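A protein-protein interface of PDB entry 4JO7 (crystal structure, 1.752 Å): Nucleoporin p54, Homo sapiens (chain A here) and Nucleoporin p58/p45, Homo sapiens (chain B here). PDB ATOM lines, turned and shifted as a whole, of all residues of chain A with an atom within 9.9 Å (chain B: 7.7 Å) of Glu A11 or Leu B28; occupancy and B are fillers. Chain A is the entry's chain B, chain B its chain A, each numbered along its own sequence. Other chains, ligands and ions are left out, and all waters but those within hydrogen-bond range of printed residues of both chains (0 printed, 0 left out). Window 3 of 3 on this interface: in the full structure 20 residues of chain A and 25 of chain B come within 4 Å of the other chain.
Among the printed residues, pairs that only touch across the chains: Leu A8 with Leu B32 (3.1 Å), Gln A19 with Tyr B21 (3.4 Å), His A15 with Tyr B21 (3.5 Å), Leu A8 with Leu B28 (3.5 Å), Glu A11 with Leu B28 (3.7 Å), His A15 with Ile B25 (3.9 Å) and Leu A16 with Ile B25 (3.9 Å).
A ring nitrogen (ND1) of His A15 lies within hydrogen-bond range of the backbone carbonyl oxygen (O) of Glu A11 (2.8 Å).
OE1 of Gln B24 sits at hydrogen-bond distance from NE2 of His A15, 2.9 Å away.
OH of Tyr B21 lies within hydrogen-bond range of OE1 of Gln A18 (2.5 Å).
Printed residues of chain A that touch a printed residue of chain B: Leu A8, Glu A11, His A15, Leu A16, Gln A18 and Gln A19.
Hydrophobic or aromatic side chains of chain A within 4 Å of the printed part of chain B: Leu A8, His A15 and Leu A16.
Printed residues of chain B that touch a printed residue of chain A: Tyr B21, Gln B24, Ile B25, Leu B28 and Leu B32.
Among the printed residues, 9 pairs touch across the chains.
Among the printed residues, no Asp or Glu carboxylate lies within 4 Å of a Lys or Arg side-chain nitrogen of the other chain.
Of chain A, only Leu A8 and Glu A11 come within 4 Å of Leu B28.
No residue of chain A comes within 4 Å of Asn B30.
Printed residues of chain B within 4 Å of Gln A19: Tyr B21.
Printed residues of chain B within 4 Å of His A15: Tyr B21, Gln B24 and Ile B25.
Of the printed residues of chain A, Tyr B21 touches His A15 (3.5 Å), Gln A18 (2.5 Å) and Gln A19 (3.4 Å).
Arg A10 touches none of the printed residues of chain B.
Arg B22 touches none of the printed residues of chain A.
The nearest residue of chain B that does not touch Glu A11 is Ile B25 (5.8 Å).
The nearest residue of chain A that does not touch Leu B28 is Ile A12 (4.4 Å).
The nearest printed residue of chain A that does not touch Leu B32 is Ile A12 (5.6 Å).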
ATOM      1  N   ASP A   5      18.595 -18.695  -7.808  1.00  0.00           N
ATOM      2  CA  ASP A   5      17.169 -18.657  -8.087  1.00  0.00           C
ATOM      3  C   ASP A   5      16.570 -20.056  -8.018  1.00  0.00           C
ATOM      4  O   ASP A   5      16.710 -20.850  -8.947  1.00  0.00           O
ATOM      5  CB  ASP A   5      16.902 -18.049  -9.464  1.00  0.00           C
ATOM      6  CG  ASP A   5      15.431 -17.833  -9.724  1.00  0.00           C
ATOM      7  OD1 ASP A   5      14.606 -18.258  -8.885  1.00  0.00           O
ATOM      8  OD2 ASP A   5      15.092 -17.237 -10.772  1.00  0.00           O
ATOM      9  N   ALA A   6      15.886 -20.336  -6.915  1.00  0.00           N
ATOM     10  CA  ALA A   6      15.282 -21.638  -6.691  1.00  0.00           C
ATOM     11  C   ALA A   6      14.128 -21.901  -7.660  1.00  0.00           C
ATOM     12  O   ALA A   6      13.847 -23.051  -7.983  1.00  0.00           O
ATOM     13  CB  ALA A   6      14.806 -21.746  -5.246  1.00  0.00           C
ATOM     14  N   ASP A   7      13.460 -20.843  -8.117  1.00  0.00           N
ATOM     15  CA  ASP A   7      12.396 -20.981  -9.117  1.00  0.00           C
ATOM     16  C   ASP A   7      12.939 -21.583 -10.409  1.00  0.00           C
ATOM     17  O   ASP A   7      12.291 -22.420 -11.040  1.00  0.00           O
ATOM     18  CB  ASP A   7      11.752 -19.628  -9.436  1.00  0.00           C
ATOM     19  CG  ASP A   7      10.599 -19.285  -8.511  1.00  0.00           C
ATOM     20  OD1 ASP A   7      10.218 -20.125  -7.672  1.00  0.00           O
ATOM     21  OD2 ASP A   7      10.052 -18.166  -8.643  1.00  0.00           O
ATOM     22  N   LEU A   8      14.132 -21.153 -10.803  1.00  0.00           N
ATOM     23  CA  LEU A   8      14.738 -21.632 -12.035  1.00  0.00           C
ATOM     24  C   LEU A   8      15.157 -23.087 -11.870  1.00  0.00           C
ATOM     25  O   LEU A   8      14.871 -23.929 -12.716  1.00  0.00           O
ATOM     26  CB  LEU A   8      15.946 -20.770 -12.401  1.00  0.00           C
ATOM     27  CG  LEU A   8      16.581 -21.044 -13.764  1.00  0.00           C
ATOM     28  CD1 LEU A   8      15.579 -20.812 -14.875  1.00  0.00           C
ATOM     29  CD2 LEU A   8      17.786 -20.158 -13.959  1.00  0.00           C
ATOM     30  N   LEU A   9      15.826 -23.388 -10.767  1.00  0.00           N
ATOM     31  CA  LEU A   9      16.242 -24.758 -10.505  1.00  0.00           C
ATOM     32  C   LEU A   9      15.026 -25.678 -10.469  1.00  0.00           C
ATOM     33  O   LEU A   9      15.062 -26.785 -11.005  1.00  0.00           O
ATOM     34  CB  LEU A   9      17.021 -24.846  -9.193  1.00  0.00           C
ATOM     35  CG  LEU A   9      17.546 -26.232  -8.825  1.00  0.00           C
ATOM     36  CD1 LEU A   9      18.421 -26.820  -9.928  1.00  0.00           C
ATOM     37  CD2 LEU A   9      18.314 -26.154  -7.519  1.00  0.00           C
ATOM     38  N   ARG A  10      13.951 -25.212  -9.843  1.00  0.00           N
ATOM     39  CA  ARG A  10      12.716 -25.987  -9.756  1.00  0.00           C
ATOM     40  C   ARG A  10      12.095 -26.214 -11.138  1.00  0.00           C
ATOM     41  O   ARG A  10      11.551 -27.283 -11.412  1.00  0.00           O
ATOM     42  CB  ARG A  10      11.728 -25.301  -8.803  1.00  0.00           C
ATOM     43  CG  ARG A  10      10.342 -25.927  -8.750  1.00  0.00           C
ATOM     44  CD  ARG A  10       9.625 -25.622  -7.428  1.00  0.00           C
ATOM     45  NE  ARG A  10       9.710 -24.210  -7.052  1.00  0.00           N
ATOM     46  CZ  ARG A  10      10.585 -23.701  -6.186  1.00  0.00           C
ATOM     47  NH1 ARG A  10      11.471 -24.478  -5.573  1.00  0.00           N
ATOM     48  NH2 ARG A  10      10.574 -22.401  -5.923  1.00  0.00           N
ATOM     49  N   GLU A  11      12.192 -25.221 -12.017  1.00  0.00           N
ATOM     50  CA  GLU A  11      11.694 -25.372 -13.381  1.00  0.00           C
ATOM     51  C   GLU A  11      12.443 -26.488 -14.117  1.00  0.00           C
ATOM     52  O   GLU A  11      11.833 -27.323 -14.794  1.00  0.00           O
ATOM     53  CB  GLU A  11      11.833 -24.051 -14.137  1.00  0.00           C
ATOM     54  CG  GLU A  11      11.133 -24.030 -15.482  1.00  0.00           C
ATOM     55  CD  GLU A  11      11.076 -22.636 -16.087  1.00  0.00           C
ATOM     56  OE1 GLU A  11      11.349 -21.654 -15.362  1.00  0.00           O
ATOM     57  OE2 GLU A  11      10.760 -22.524 -17.289  1.00  0.00           O
ATOM     58  N   ILE A  12      13.764 -26.494 -13.984  1.00  0.00           N
ATOM     59  CA  ILE A  12      14.597 -27.547 -14.562  1.00  0.00           C
ATOM     60  C   ILE A  12      14.229 -28.900 -13.952  1.00  0.00           C
ATOM     61  O   ILE A  12      14.049 -29.890 -14.663  1.00  0.00           O
ATOM     62  CB  ILE A  12      16.096 -27.270 -14.326  1.00  0.00           C
ATOM     63  CG1 ILE A  12      16.526 -25.997 -15.063  1.00  0.00           C
ATOM     64  CG2 ILE A  12      16.944 -28.463 -14.774  1.00  0.00           C
ATOM     65  CD1 ILE A  12      17.913 -25.516 -14.679  1.00  0.00           C
ATOM     66  N   LYS A  13      14.105 -28.928 -12.630  1.00  0.00           N
ATOM     67  CA  LYS A  13      13.778 -30.146 -11.903  1.00  0.00           C
ATOM     68  C   LYS A  13      12.463 -30.754 -12.387  1.00  0.00           C
ATOM     69  O   LYS A  13      12.340 -31.974 -12.503  1.00  0.00           O
ATOM     70  CB  LYS A  13      13.706 -29.850 -10.401  1.00  0.00           C
ATOM     71  CG  LYS A  13      13.356 -31.047  -9.525  1.00  0.00           C
ATOM     72  CD  LYS A  13      11.867 -31.168  -9.293  1.00  0.00           C
ATOM     73  CE  LYS A  13      11.553 -32.035  -8.080  1.00  0.00           C
ATOM     74  NZ  LYS A  13      11.872 -31.352  -6.792  1.00  0.00           N
ATOM     75  N   GLN A  14      11.487 -29.898 -12.676  1.00  0.00           N
ATOM     76  CA  GLN A  14      10.156 -30.352 -13.077  1.00  0.00           C
ATOM     77  C   GLN A  14      10.160 -30.996 -14.463  1.00  0.00           C
ATOM     78  O   GLN A  14       9.427 -31.953 -14.708  1.00  0.00           O
ATOM     79  CB  GLN A  14       9.166 -29.184 -13.045  1.00  0.00           C
ATOM     80  CG  GLN A  14       8.762 -28.756 -11.638  1.00  0.00           C
ATOM     81  CD  GLN A  14       8.047 -27.412 -11.604  1.00  0.00           C
ATOM     82  OE1 GLN A  14       7.862 -26.767 -12.632  1.00  0.00           O
ATOM     83  NE2 GLN A  14       7.649 -26.986 -10.413  1.00  0.00           N
ATOM     84  N   HIS A  15      11.013 -30.486 -15.344  1.00  0.00           N
ATOM     85  CA  HIS A  15      11.185 -31.066 -16.659  1.00  0.00           C
ATOM     86  C   HIS A  15      11.747 -32.451 -16.539  1.00  0.00           C
ATOM     87  O   HIS A  15      11.240 -33.403 -17.173  1.00  0.00           O
ATOM     88  CB  HIS A  15      12.111 -30.200 -17.505  1.00  0.00           C
ATOM     89  CG  HIS A  15      11.441 -28.976 -18.080  1.00  0.00           C
ATOM     90  ND1 HIS A  15      11.587 -27.751 -17.542  1.00  0.00           N
ATOM     91  CD2 HIS A  15      10.602 -28.824 -19.183  1.00  0.00           C
ATOM     92  CE1 HIS A  15      10.880 -26.860 -18.262  1.00  0.00           C
ATOM     93  NE2 HIS A  15      10.278 -27.517 -19.266  1.00  0.00           N
ATOM     94  N   LEU A  16      12.795 -32.599 -15.731  1.00  0.00           N
ATOM     95  CA  LEU A  16      13.419 -33.906 -15.528  1.00  0.00           C
ATOM     96  C   LEU A  16      12.444 -34.880 -14.864  1.00  0.00           C
ATOM     97  O   LEU A  16      12.376 -36.048 -15.235  1.00  0.00           O
ATOM     98  CB  LEU A  16      14.702 -33.781 -14.706  1.00  0.00           C
ATOM     99  CG  LEU A  16      15.795 -32.885 -15.297  1.00  0.00           C
ATOM    100  CD1 LEU A  16      17.066 -32.987 -14.461  1.00  0.00           C
ATOM    101  CD2 LEU A  16      16.078 -33.229 -16.748  1.00  0.00           C
ATOM    102  N   LYS A  17      11.672 -34.388 -13.902  1.00  0.00           N
ATOM    103  CA  LYS A  17      10.681 -35.208 -13.214  1.00  0.00           C
ATOM    104  C   LYS A  17       9.671 -35.808 -14.197  1.00  0.00           C
ATOM    105  O   LYS A  17       9.314 -36.984 -14.109  1.00  0.00           O
ATOM    106  CB  LYS A  17       9.955 -34.364 -12.165  1.00  0.00           C
ATOM    107  CG  LYS A  17       8.835 -35.092 -11.430  1.00  0.00           C
ATOM    108  CD  LYS A  17       9.360 -36.258 -10.606  1.00  0.00           C
ATOM    109  CE  LYS A  17       8.229 -36.939  -9.840  1.00  0.00           C
ATOM    110  NZ  LYS A  17       8.674 -38.199  -9.187  1.00  0.00           N
ATOM    111  N   GLN A  18       9.214 -35.001 -15.141  1.00  0.00           N
ATOM    112  CA  GLN A  18       8.272 -35.494 -16.131  1.00  0.00           C
ATOM    113  C   GLN A  18       8.904 -36.613 -16.970  1.00  0.00           C
ATOM    114  O   GLN A  18       8.224 -37.560 -17.362  1.00  0.00           O
ATOM    115  CB  GLN A  18       7.786 -34.355 -17.022  1.00  0.00           C
ATOM    116  CG  GLN A  18       6.637 -34.742 -17.936  1.00  0.00           C
ATOM    117  CD  GLN A  18       5.898 -33.535 -18.487  1.00  0.00           C
ATOM    118  OE1 GLN A  18       6.210 -32.395 -18.146  1.00  0.00           O
ATOM    119  NE2 GLN A  18       4.911 -33.783 -19.337  1.00  0.00           N
ATOM    120  N   GLN A  19      10.203 -36.510 -17.243  1.00  0.00           N
ATOM    121  CA  GLN A  19      10.895 -37.566 -17.990  1.00  0.00           C
ATOM    122  C   GLN A  19      11.046 -38.830 -17.153  1.00  0.00           C
ATOM    123  O   GLN A  19      10.927 -39.948 -17.666  1.00  0.00           O
ATOM    124  CB  GLN A  19      12.266 -37.084 -18.457  1.00  0.00           C
ATOM    125  CG  GLN A  19      12.185 -35.867 -19.341  1.00  0.00           C
ATOM    126  CD  GLN A  19      13.541 -35.326 -19.701  1.00  0.00           C
ATOM    127  OE1 GLN A  19      14.576 -35.752 -19.168  1.00  0.00           O
ATOM    128  NE2 GLN A  19      13.552 -34.392 -20.623  1.00  0.00           N
ATOM    129  N   TYR B  21      12.418 -30.688 -24.256  1.00  0.00           N
ATOM    130  CA  TYR B  21      12.872 -30.282 -22.929  1.00  0.00           C
ATOM    131  C   TYR B  21      14.360 -29.962 -22.917  1.00  0.00           C
ATOM    132  O   TYR B  21      14.815 -29.121 -22.142  1.00  0.00           O
ATOM    133  CB  TYR B  21      12.555 -31.359 -21.891  1.00  0.00           C
ATOM    134  CG  TYR B  21      11.105 -31.389 -21.467  1.00  0.00           C
ATOM    135  CD1 TYR B  21      10.153 -30.606 -22.111  1.00  0.00           C
ATOM    136  CD2 TYR B  21      10.689 -32.181 -20.407  1.00  0.00           C
ATOM    137  CE1 TYR B  21       8.830 -30.621 -21.717  1.00  0.00           C
ATOM    138  CE2 TYR B  21       9.367 -32.203 -20.008  1.00  0.00           C
ATOM    139  CZ  TYR B  21       8.443 -31.419 -20.665  1.00  0.00           C
ATOM    140  OH  TYR B  21       7.125 -31.436 -20.270  1.00  0.00           O
ATOM    141  N   ARG B  22      15.115 -30.628 -23.780  1.00  0.00           N
ATOM    142  CA  ARG B  22      16.551 -30.407 -23.846  1.00  0.00           C
ATOM    143  C   ARG B  22      16.815 -28.961 -24.236  1.00  0.00           C
ATOM    144  O   ARG B  22      17.700 -28.308 -23.682  1.00  0.00           O
ATOM    145  CB  ARG B  22      17.189 -31.363 -24.856  1.00  0.00           C
ATOM    146  CG  ARG B  22      18.702 -31.266 -24.946  1.00  0.00           C
ATOM    147  CD  ARG B  22      19.263 -32.365 -25.836  1.00  0.00           C
ATOM    148  NE  ARG B  22      20.322 -31.883 -26.719  1.00  0.00           N
ATOM    149  CZ  ARG B  22      21.580 -31.674 -26.345  1.00  0.00           C
ATOM    150  NH1 ARG B  22      21.957 -31.898 -25.092  1.00  0.00           N
ATOM    151  NH2 ARG B  22      22.468 -31.235 -27.227  1.00  0.00           N
ATOM    152  N   GLN B  23      16.024 -28.458 -25.177  1.00  0.00           N
ATOM    153  CA  GLN B  23      16.181 -27.090 -25.651  1.00  0.00           C
ATOM    154  C   GLN B  23      15.683 -26.095 -24.611  1.00  0.00           C
ATOM    155  O   GLN B  23      16.318 -25.070 -24.371  1.00  0.00           O
ATOM    156  CB  GLN B  23      15.434 -26.893 -26.969  1.00  0.00           C
ATOM    157  CG  GLN B  23      15.511 -25.477 -27.515  1.00  0.00           C
ATOM    158  CD  GLN B  23      16.939 -25.007 -27.711  1.00  0.00           C
ATOM    159  OE1 GLN B  23      17.451 -24.195 -26.937  1.00  0.00           O
ATOM    160  NE2 GLN B  23      17.592 -25.513 -28.753  1.00  0.00           N
ATOM    161  N   GLN B  24      14.549 -26.408 -23.994  1.00  0.00           N
ATOM    162  CA  GLN B  24      13.950 -25.533 -22.995  1.00  0.00           C
ATOM    163  C   GLN B  24      14.880 -25.352 -21.796  1.00  0.00           C
ATOM    164  O   GLN B  24      14.975 -24.262 -21.228  1.00  0.00           O
ATOM    165  CB  GLN B  24      12.599 -26.097 -22.549  1.00  0.00           C
ATOM    166  CG  GLN B  24      11.578 -26.182 -23.676  1.00  0.00           C
ATOM    167  CD  GLN B  24      10.261 -26.791 -23.236  1.00  0.00           C
ATOM    168  OE1 GLN B  24       9.905 -26.749 -22.058  1.00  0.00           O
ATOM    169  NE2 GLN B  24       9.532 -27.365 -24.184  1.00  0.00           N
ATOM    170  N   ILE B  25      15.573 -26.421 -21.417  1.00  0.00           N
ATOM    171  CA  ILE B  25      16.505 -26.362 -20.294  1.00  0.00           C
ATOM    172  C   ILE B  25      17.785 -25.631 -20.686  1.00  0.00           C
ATOM    173  O   ILE B  25      18.353 -24.887 -19.889  1.00  0.00           O
ATOM    174  CB  ILE B  25      16.839 -27.766 -19.767  1.00  0.00           C
ATOM    175  CG1 ILE B  25      15.632 -28.331 -19.014  1.00  0.00           C
ATOM    176  CG2 ILE B  25      18.059 -27.714 -18.849  1.00  0.00           C
ATOM    177  CD1 ILE B  25      15.827 -29.738 -18.501  1.00  0.00           C
ATOM    178  N   GLU B  26      18.229 -25.830 -21.923  1.00  0.00           N
ATOM    179  CA  GLU B  26      19.430 -25.163 -22.408  1.00  0.00           C
ATOM    180  C   GLU B  26      19.240 -23.649 -22.422  1.00  0.00           C
ATOM    181  O   GLU B  26      20.178 -22.899 -22.155  1.00  0.00           O
ATOM    182  CB  GLU B  26      19.794 -25.659 -23.809  1.00  0.00           C
ATOM    183  CG  GLU B  26      21.074 -25.053 -24.366  1.00  0.00           C
ATOM    184  CD  GLU B  26      22.293 -25.362 -23.514  1.00  0.00           C
ATOM    185  OE1 GLU B  26      22.211 -26.271 -22.660  1.00  0.00           O
ATOM    186  OE2 GLU B  26      23.334 -24.693 -23.698  1.00  0.00           O
ATOM    187  N   GLU B  27      18.026 -23.201 -22.721  1.00  0.00           N
ATOM    188  CA  GLU B  27      17.743 -21.771 -22.762  1.00  0.00           C
ATOM    189  C   GLU B  27      17.630 -21.198 -21.353  1.00  0.00           C
ATOM    190  O   GLU B  27      17.954 -20.033 -21.121  1.00  0.00           O
ATOM    191  CB  GLU B  27      16.461 -21.490 -23.546  1.00  0.00           C
ATOM    192  CG  GLU B  27      16.141 -20.007 -23.687  1.00  0.00           C
ATOM    193  CD  GLU B  27      17.269 -19.228 -24.339  1.00  0.00           C
ATOM    194  OE1 GLU B  27      18.144 -19.862 -24.968  1.00  0.00           O
ATOM    195  OE2 GLU B  27      17.283 -17.983 -24.218  1.00  0.00           O
ATOM    196  N   LEU B  28      17.160 -22.017 -20.417  1.00  0.00           N
ATOM    197  CA  LEU B  28      17.117 -21.623 -19.014  1.00  0.00           C
ATOM    198  C   LEU B  28      18.530 -21.456 -18.467  1.00  0.00           C
ATOM    199  O   LEU B  28      18.768 -20.635 -17.583  1.00  0.00           O
ATOM    200  CB  LEU B  28      16.370 -22.667 -18.182  1.00  0.00           C
ATOM    201  CG  LEU B  28      14.887 -22.441 -17.870  1.00  0.00           C
ATOM    202  CD1 LEU B  28      14.252 -21.400 -18.782  1.00  0.00           C
ATOM    203  CD2 LEU B  28      14.136 -23.758 -17.957  1.00  0.00           C
ATOM    204  N   GLU B  29      19.467 -22.228 -19.007  1.00  0.00           N
ATOM    205  CA  GLU B  29      20.826 -22.265 -18.474  1.00  0.00           C
ATOM    206  C   GLU B  29      21.674 -21.073 -18.900  1.00  0.00           C
ATOM    207  O   GLU B  29      22.345 -20.461 -18.072  1.00  0.00           O
ATOM    208  CB  GLU B  29      21.522 -23.559 -18.886  1.00  0.00           C
ATOM    209  CG  GLU B  29      21.082 -24.762 -18.085  1.00  0.00           C
ATOM    210  CD  GLU B  29      21.779 -26.025 -18.528  1.00  0.00           C
ATOM    211  OE1 GLU B  29      22.040 -26.162 -19.743  1.00  0.00           O
ATOM    212  OE2 GLU B  29      22.074 -26.870 -17.660  1.00  0.00           O
ATOM    213  N   ASN B  30      21.652 -20.738 -20.185  1.00  0.00           N
ATOM    214  CA  ASN B  30      22.422 -19.591 -20.657  1.00  0.00           C
ATOM    215  C   ASN B  30      21.980 -18.287 -19.988  1.00  0.00           C
ATOM    216  O   ASN B  30      22.640 -17.257 -20.120  1.00  0.00           O
ATOM    217  CB  ASN B  30      22.573 -19.601 -22.184  1.00  0.00           C
ATOM    218  CG  ASN B  30      21.309 -20.030 -22.899  1.00  0.00           C
ATOM    219  OD1 ASN B  30      20.216 -19.553 -22.597  1.00  0.00           O
ATOM    220  ND2 ASN B  30      21.455 -20.948 -23.850  1.00  0.00           N
ATOM    221  N   HIS B  31      20.881 -18.355 -19.240  1.00  0.00           N
ATOM    222  CA  HIS B  31      20.369 -17.206 -18.514  1.00  0.00           C
ATOM    223  C   HIS B  31      20.714 -17.281 -17.052  1.00  0.00           C
ATOM    224  O   HIS B  31      20.079 -16.610 -16.209  1.00  0.00           O
ATOM    225  CB  HIS B  31      18.858 -17.102 -18.689  1.00  0.00           C
ATOM    226  CG  HIS B  31      18.426 -15.963 -19.582  1.00  0.00           C
ATOM    227  ND1 HIS B  31      17.268 -15.304 -19.404  1.00  0.00           N
ATOM    228  CD2 HIS B  31      19.046 -15.377 -20.685  1.00  0.00           C
ATOM    229  CE1 HIS B  31      17.148 -14.345 -20.341  1.00  0.00           C
ATOM    230  NE2 HIS B  31      18.237 -14.392 -21.125  1.00  0.00           N
ATOM    231  N   LEU B  32      21.720 -18.087 -16.725  1.00  0.00           N
ATOM    232  CA  LEU B  32      22.196 -18.228 -15.353  1.00  0.00           C
ATOM    233  C   LEU B  32      23.227 -17.160 -15.033  1.00  0.00           C
ATOM    234  O   LEU B  32      24.147 -16.929 -15.814  1.00  0.00           O
ATOM    235  CB  LEU B  32      22.847 -19.597 -15.150  1.00  0.00           C
ATOM    236  CG  LEU B  32      21.958 -20.777 -14.763  1.00  0.00           C
ATOM    237  CD1 LEU B  32      20.545 -20.569 -15.236  1.00  0.00           C
ATOM    238  CD2 LEU B  32      22.533 -22.046 -15.345  1.00  0.00           C
ATOM    239  N   ALA B  33      23.083 -16.522 -13.875  1.00  0.00           N
ATOM    240  CA  ALA B  33      24.067 -15.554 -13.406  1.00  0.00           C
ATOM    241  C   ALA B  33      24.967 -16.227 -12.376  1.00  0.00           C
ATOM    242  O   ALA B  33      24.552 -16.467 -11.242  1.00  0.00           O
ATOM    243  CB  ALA B  33      23.375 -14.345 -12.800  1.00  0.00           C
